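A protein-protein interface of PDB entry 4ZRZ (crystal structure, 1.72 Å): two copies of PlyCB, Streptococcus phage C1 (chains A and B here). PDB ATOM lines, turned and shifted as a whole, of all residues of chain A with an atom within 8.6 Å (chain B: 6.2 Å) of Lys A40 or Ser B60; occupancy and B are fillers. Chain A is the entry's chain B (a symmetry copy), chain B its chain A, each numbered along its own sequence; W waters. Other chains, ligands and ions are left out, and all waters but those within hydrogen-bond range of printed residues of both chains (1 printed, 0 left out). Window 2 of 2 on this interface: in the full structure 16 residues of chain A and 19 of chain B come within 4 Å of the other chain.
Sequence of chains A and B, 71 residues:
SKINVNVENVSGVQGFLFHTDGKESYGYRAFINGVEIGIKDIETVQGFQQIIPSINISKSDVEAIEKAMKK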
ATOM      1  N   LEU A  17     -15.981   6.744  23.559  1.00  0.00           N
ATOM      2  CA  LEU A  17     -15.536   8.113  23.766  1.00  0.00           C
ATOM      3  C   LEU A  17     -16.720   8.926  24.284  1.00  0.00           C
ATOM      4  O   LEU A  17     -17.867   8.743  23.844  1.00  0.00           O
ATOM      5  CB  LEU A  17     -15.073   8.711  22.455  1.00  0.00           C
ATOM      6  CG  LEU A  17     -13.810   8.094  21.834  1.00  0.00           C
ATOM      7  CD1 LEU A  17     -13.781   8.196  20.337  1.00  0.00           C
ATOM      8  CD2 LEU A  17     -12.614   8.827  22.408  1.00  0.00           C
ATOM      9  N   TYR A  26     -15.021  19.364  29.013  1.00  0.00           N
ATOM     10  CA  TYR A  26     -14.019  18.587  29.733  1.00  0.00           C
ATOM     11  C   TYR A  26     -13.103  17.827  28.746  1.00  0.00           C
ATOM     12  O   TYR A  26     -12.373  16.924  29.142  1.00  0.00           O
ATOM     13  CB  TYR A  26     -14.660  17.662  30.788  1.00  0.00           C
ATOM     14  CG  TYR A  26     -15.722  16.731  30.215  1.00  0.00           C
ATOM     15  CD1 TYR A  26     -15.356  15.563  29.551  1.00  0.00           C
ATOM     16  CD2 TYR A  26     -17.084  17.025  30.327  1.00  0.00           C
ATOM     17  CE1 TYR A  26     -16.313  14.708  29.011  1.00  0.00           C
ATOM     18  CE2 TYR A  26     -18.053  16.174  29.782  1.00  0.00           C
ATOM     19  CZ  TYR A  26     -17.648  15.002  29.135  1.00  0.00           C
ATOM     20  OH  TYR A  26     -18.554  14.143  28.555  1.00  0.00           O
ATOM     21  N   GLY A  27     -13.127  18.234  27.488  1.00  0.00           N
ATOM     22  CA  GLY A  27     -12.396  17.576  26.411  1.00  0.00           C
ATOM     23  C   GLY A  27     -13.028  16.229  26.111  1.00  0.00           C
ATOM     24  O   GLY A  27     -14.211  16.009  26.409  1.00  0.00           O
ATOM     25  N   TYR A  28     -12.248  15.346  25.489  1.00  0.00           N
ATOM     26  CA  TYR A  28     -12.698  13.973  25.207  1.00  0.00           C
ATOM     27  C   TYR A  28     -12.120  13.027  26.235  1.00  0.00           C
ATOM     28  O   TYR A  28     -10.955  13.160  26.689  1.00  0.00           O
ATOM     29  CB  TYR A  28     -12.327  13.543  23.789  1.00  0.00           C
ATOM     30  CG  TYR A  28     -13.220  14.066  22.704  1.00  0.00           C
ATOM     31  CD1 TYR A  28     -14.180  13.246  22.102  1.00  0.00           C
ATOM     32  CD2 TYR A  28     -13.088  15.359  22.240  1.00  0.00           C
ATOM     33  CE1 TYR A  28     -14.989  13.713  21.091  1.00  0.00           C
ATOM     34  CE2 TYR A  28     -13.871  15.837  21.218  1.00  0.00           C
ATOM     35  CZ  TYR A  28     -14.825  15.021  20.646  1.00  0.00           C
ATOM     36  OH  TYR A  28     -15.603  15.495  19.627  1.00  0.00           O
ATOM     37  N   ARG A  29     -12.973  12.105  26.688  1.00  0.00           N
ATOM     38  CA  ARG A  29     -12.547  11.043  27.573  1.00  0.00           C
ATOM     39  C   ARG A  29     -13.012   9.753  26.926  1.00  0.00           C
ATOM     40  O   ARG A  29     -13.699   9.773  25.901  1.00  0.00           O
ATOM     41  CB  ARG A  29     -13.132  11.205  28.975  1.00  0.00           C
ATOM     42  CG  ARG A  29     -12.634  12.450  29.733  1.00  0.00           C
ATOM     43  CD  ARG A  29     -12.900  12.311  31.215  1.00  0.00           C
ATOM     44  NE  ARG A  29     -12.629  13.540  31.969  1.00  0.00           N
ATOM     45  CZ  ARG A  29     -13.058  13.788  33.211  1.00  0.00           C
ATOM     46  NH1 ARG A  29     -13.815  12.911  33.885  1.00  0.00           N
ATOM     47  NH2 ARG A  29     -12.745  14.941  33.793  1.00  0.00           N
ATOM     48  N   ILE A  37      -9.897   7.026  30.691  1.00  0.00           N
ATOM     49  CA  ILE A  37      -8.738   7.841  30.309  1.00  0.00           C
ATOM     50  C   ILE A  37      -9.165   9.161  29.699  1.00  0.00           C
ATOM     51  O   ILE A  37     -10.289   9.315  29.193  1.00  0.00           O
ATOM     52  CB  ILE A  37      -7.795   7.144  29.287  1.00  0.00           C
ATOM     53  CG1 ILE A  37      -8.525   6.775  28.000  1.00  0.00           C
ATOM     54  CG2 ILE A  37      -7.138   5.924  29.912  1.00  0.00           C
ATOM     55  CD1 ILE A  37      -7.594   6.255  26.921  1.00  0.00           C
ATOM     56  N   GLY A  38      -8.239  10.116  29.750  1.00  0.00           N
ATOM     57  CA  GLY A  38      -8.373  11.351  29.022  1.00  0.00           C
ATOM     58  C   GLY A  38      -7.722  11.155  27.655  1.00  0.00           C
ATOM     59  O   GLY A  38      -6.747  10.419  27.515  1.00  0.00           O
ATOM     60  N   ILE A  39      -8.272  11.805  26.648  1.00  0.00           N
ATOM     61  CA  ILE A  39      -7.652  11.846  25.318  1.00  0.00           C
ATOM     62  C   ILE A  39      -7.227  13.289  25.067  1.00  0.00           C
ATOM     63  O   ILE A  39      -8.058  14.203  25.145  1.00  0.00           O
ATOM     64  CB  ILE A  39      -8.646  11.456  24.201  1.00  0.00           C
ATOM     65  CG1 ILE A  39      -9.326  10.123  24.478  1.00  0.00           C
ATOM     66  CG2 ILE A  39      -7.961  11.457  22.843  1.00  0.00           C
ATOM     67  CD1 ILE A  39      -8.412   8.936  24.564  1.00  0.00           C
ATOM     68  N   LYS A  40      -5.950  13.489  24.743  1.00  0.00           N
ATOM     69  CA  LYS A  40      -5.363  14.825  24.558  1.00  0.00           C
ATOM     70  C   LYS A  40      -5.536  15.391  23.138  1.00  0.00           C
ATOM     71  O   LYS A  40      -5.769  16.588  22.971  1.00  0.00           O
ATOM     72  CB  LYS A  40      -3.865  14.792  24.890  1.00  0.00           C
ATOM     73  CG  LYS A  40      -3.477  14.274  26.262  1.00  0.00           C
ATOM     74  CD  LYS A  40      -1.954  14.106  26.306  1.00  0.00           C
ATOM     75  CE  LYS A  40      -1.404  13.542  27.614  1.00  0.00           C
ATOM     76  NZ  LYS A  40      -2.326  13.753  28.759  1.00  0.00           N
ATOM     77  N   ASP A  41      -5.492  14.545  22.111  1.00  0.00           N
ATOM     78  CA  ASP A  41      -5.328  15.013  20.723  1.00  0.00           C
ATOM     79  C   ASP A  41      -6.465  14.550  19.864  1.00  0.00           C
ATOM     80  O   ASP A  41      -6.856  13.361  19.930  1.00  0.00           O
ATOM     81  CB  ASP A  41      -4.018  14.452  20.153  1.00  0.00           C
ATOM     82  CG  ASP A  41      -3.548  15.164  18.873  1.00  0.00           C
ATOM     83  OD1 ASP A  41      -4.241  15.261  17.817  1.00  0.00           O
ATOM     84  OD2 ASP A  41      -2.388  15.613  18.908  1.00  0.00           O
ATOM     85  N   ILE A  42      -6.964  15.417  18.984  1.00  0.00           N
ATOM     86  CA  ILE A  42      -8.105  15.030  18.130  1.00  0.00           C
ATOM     87  C   ILE A  42      -7.760  13.898  17.144  1.00  0.00           C
ATOM     88  O   ILE A  42      -8.638  13.155  16.721  1.00  0.00           O
ATOM     89  CB  ILE A  42      -8.662  16.241  17.365  1.00  0.00           C
ATOM     90  CG1 ILE A  42     -10.073  15.990  16.830  1.00  0.00           C
ATOM     91  CG2 ILE A  42      -7.725  16.671  16.241  1.00  0.00           C
ATOM     92  CD1 ILE A  42     -11.175  15.829  17.846  1.00  0.00           C
ATOM     93  N   GLU A  43      -6.481  13.781  16.757  1.00  0.00           N
ATOM     94  CA  GLU A  43      -6.078  12.622  15.942  1.00  0.00           C
ATOM     95  C   GLU A  43      -6.478  11.308  16.609  1.00  0.00           C
ATOM     96  O   GLU A  43      -6.993  10.401  15.943  1.00  0.00           O
ATOM     97  CB  GLU A  43      -4.563  12.641  15.686  1.00  0.00           C
ATOM     98  CG  GLU A  43      -4.105  11.432  14.871  1.00  0.00           C
ATOM     99  CD  GLU A  43      -2.614  11.374  14.630  1.00  0.00           C
ATOM    100  OE1 GLU A  43      -1.818  11.818  15.513  1.00  0.00           O
ATOM    101  OE2 GLU A  43      -2.240  10.787  13.583  1.00  0.00           O
ATOM    102  N   THR A  44      -6.235  11.212  17.909  1.00  0.00           N
ATOM    103  CA  THR A  44      -6.522  10.012  18.676  1.00  0.00           C
ATOM    104  C   THR A  44      -8.046   9.794  18.787  1.00  0.00           C
ATOM    105  O   THR A  44      -8.542   8.683  18.669  1.00  0.00           O
ATOM    106  CB  THR A  44      -5.922  10.136  20.074  1.00  0.00           C
ATOM    107  OG1 THR A  44      -4.532  10.450  19.954  1.00  0.00           O
ATOM    108  CG2 THR A  44      -6.099   8.846  20.882  1.00  0.00           C
ATOM    109  N   VAL A  45      -8.790  10.865  18.991  1.00  0.00           N
ATOM    110  CA  VAL A  45     -10.258  10.778  18.981  1.00  0.00           C
ATOM    111  C   VAL A  45     -10.762  10.174  17.669  1.00  0.00           C
ATOM    112  O   VAL A  45     -11.585   9.253  17.682  1.00  0.00           O
ATOM    113  CB  VAL A  45     -10.927  12.176  19.194  1.00  0.00           C
ATOM    114  CG1 VAL A  45     -12.445  12.059  19.055  1.00  0.00           C
ATOM    115  CG2 VAL A  45     -10.588  12.675  20.583  1.00  0.00           C
ATOM    116  N   ILE B  57      -3.128   7.251  16.573  1.00  0.00           N
ATOM    117  CA  ILE B  57      -3.010   7.642  17.969  1.00  0.00           C
ATOM    118  C   ILE B  57      -1.856   8.621  18.038  1.00  0.00           C
ATOM    119  O   ILE B  57      -0.763   8.292  17.603  1.00  0.00           O
ATOM    120  CB  ILE B  57      -2.732   6.460  18.910  1.00  0.00           C
ATOM    121  CG1 ILE B  57      -3.836   5.390  18.796  1.00  0.00           C
ATOM    122  CG2 ILE B  57      -2.582   6.920  20.344  1.00  0.00           C
ATOM    123  CD1 ILE B  57      -3.647   4.215  19.754  1.00  0.00           C
ATOM    124  N   SER B  58      -2.121   9.812  18.557  1.00  0.00           N
ATOM    125  CA  SER B  58      -1.044  10.829  18.745  1.00  0.00           C
ATOM    126  C   SER B  58       0.023  10.326  19.705  1.00  0.00           C
ATOM    127  O   SER B  58      -0.238   9.553  20.644  1.00  0.00           O
ATOM    128  CB  SER B  58      -1.612  12.147  19.304  1.00  0.00           C
ATOM    129  OG  SER B  58      -1.926  12.013  20.680  1.00  0.00           O
ATOM    130  N   LYS B  59       1.266  10.754  19.505  1.00  0.00           N
ATOM    131  CA  LYS B  59       2.307  10.363  20.455  1.00  0.00           C
ATOM    132  C   LYS B  59       1.939  10.686  21.897  1.00  0.00           C
ATOM    133  O   LYS B  59       2.131   9.865  22.763  1.00  0.00           O
ATOM    134  CB  LYS B  59       3.639  11.040  20.106  1.00  0.00           C
ATOM    135  CG  LYS B  59       4.788  10.566  20.993  1.00  0.00           C
ATOM    136  CD  LYS B  59       6.118  11.106  20.517  1.00  0.00           C
ATOM    137  CE  LYS B  59       7.212  10.858  21.550  1.00  0.00           C
ATOM    138  NZ  LYS B  59       8.492  11.480  21.118  1.00  0.00           N
ATOM    139  N   SER B  60       1.341  11.860  22.149  1.00  0.00           N
ATOM    140  CA  SER B  60       0.960  12.268  23.508  1.00  0.00           C
ATOM    141  C   SER B  60      -0.083  11.361  24.202  1.00  0.00           C
ATOM    142  O   SER B  60      -0.137  11.333  25.420  1.00  0.00           O
ATOM    143  CB  SER B  60       0.473  13.737  23.548  1.00  0.00           C
ATOM    144  OG  SER B  60      -0.736  13.928  22.808  1.00  0.00           O
ATOM    145  N   ASP B  61      -0.870  10.633  23.426  1.00  0.00           N
ATOM    146  CA  ASP B  61      -1.900   9.729  23.942  1.00  0.00           C
ATOM    147  C   ASP B  61      -1.482   8.270  24.087  1.00  0.00           C
ATOM    148  O   ASP B  61      -2.215   7.483  24.696  1.00  0.00           O
ATOM    149  CB  ASP B  61      -3.135   9.813  23.048  1.00  0.00           C
ATOM    150  CG  ASP B  61      -3.915  11.082  23.276  1.00  0.00           C
ATOM    151  OD1 ASP B  61      -4.046  11.443  24.448  1.00  0.00           O
ATOM    152  OD2 ASP B  61      -4.388  11.696  22.301  1.00  0.00           O
ATOM    153  N   VAL B  62      -0.321   7.909  23.553  1.00  0.00           N
ATOM    154  CA  VAL B  62       0.120   6.507  23.593  1.00  0.00           C
ATOM    155  C   VAL B  62       0.158   5.998  25.049  1.00  0.00           C
ATOM    156  O   VAL B  62      -0.386   4.928  25.332  1.00  0.00           O
ATOM    157  CB  VAL B  62       1.473   6.298  22.867  1.00  0.00           C
ATOM    158  CG1 VAL B  62       2.006   4.892  23.125  1.00  0.00           C
ATOM    159  CG2 VAL B  62       1.291   6.454  21.362  1.00  0.00           C
ATOM    160  N   GLU B  63       0.733   6.793  25.958  1.00  0.00           N
ATOM    161  CA  GLU B  63       0.893   6.404  27.383  1.00  0.00           C
ATOM    162  C   GLU B  63      -0.433   6.003  28.037  1.00  0.00           C
ATOM    163  O   GLU B  63      -0.514   4.959  28.678  1.00  0.00           O
ATOM    164  CB  GLU B  63       1.576   7.521  28.194  1.00  0.00           C
ATOM    165  CG  GLU B  63       2.035   7.086  29.592  1.00  0.00           C
ATOM    166  CD  GLU B  63       2.417   8.241  30.519  1.00  0.00           C
ATOM    167  OE1 GLU B  63       2.594   7.963  31.722  1.00  0.00           O
ATOM    168  OE2 GLU B  63       2.534   9.406  30.075  1.00  0.00           O
ATOM    169  N   ALA B  64      -1.468   6.821  27.848  1.00  0.00           N
ATOM    170  CA  ALA B  64      -2.807   6.526  28.369  1.00  0.00           C
ATOM    171  C   ALA B  64      -3.440   5.268  27.755  1.00  0.00           C
ATOM    172  O   ALA B  64      -4.067   4.496  28.474  1.00  0.00           O
ATOM    173  CB  ALA B  64      -3.724   7.720  28.167  1.00  0.00           C
HETATM  174  O   HOH W   1      -4.047  10.785  26.953  1.00  0.00           O
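OD2 of Asp B61 sits at hydrogen-bond distance from OG1 of Thr A44, 2.7 Å away. The side-chain carboxylate of Asp B61 sits at hydrogen-bond distance from the backbone NH of Lys A40 (2.8 Å). The backbone NH (N) of Asp A41 lies within hydrogen-bond range of the side-chain carboxylate (OD2) of Asp B61 (3.1 Å). N of Ser B58 is in hydrogen-bond range of OG1 of Thr A44 (2.9 Å).
The side-chain hydroxyl of Ser B58 lies within hydrogen-bond range of the side-chain carboxylate of Asp B61 (3.0 Å). The side-chain hydroxyl (OG) of Ser B60 sits at hydrogen-bond distance from the side-chain hydroxyl (OG) of Ser B58, 3.1 Å away. The side-chain carboxylate (OD1) of Asp A41 is in hydrogen-bond range of the backbone NH (N) of Glu A43, 2.9 Å away. The backbone carbonyl oxygen (O) of Tyr A28 is in hydrogen-bond range of the backbone NH (N) of Ile A39.
Among the printed residues, pairs that only touch across the chains: Asp A41 with Ser B58 (3.3 Å), Lys A40 with Ser B60 (3.4 Å), Glu A43 with Ser B58 (3.5 Å), Ile A39 with Asp B61 (3.6 Å), Ile A37 with Ala B64 (3.7 Å) and Thr A44 with Ile B57 (3.8 Å).
Lys A40 touches two residues of chain B. Ser B60 touches just one residue of chain A: Lys A40. Printed residues of chain B within 4 Å of Glu A43: Ser B58. Of the printed residues of chain A, Ala B64 touches Ile A37. Printed residues of chain B within 4 Å of Ile A39: Asp B61 (3.6 Å). Of the printed residues of chain B, Asp A41 touches Ser B58 and Asp B61. Of the printed residues of chain A, Ile B57 touches Thr A44 (3.8 Å). The nearest printed residue of chain A that does not touch Ala B64 is Gly A38 (4.1 Å).
Of the 14 printed residues of chain A, 6 touch a printed residue of chain B. Hydrophobic or aromatic side chains of chain A within 4 Å of the printed part of chain B: Ile A37 and Ile A39. Of the 8 printed residues of chain B, 5 touch a printed residue of chain A.
No position is printed for both chains.
Water W1 lies within hydrogen-bond range of the side-chain carboxylate (OD1) of Asp B61 (2.6 Å) and the backbone carbonyl oxygen (O) of Gly A38 (2.8 Å).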
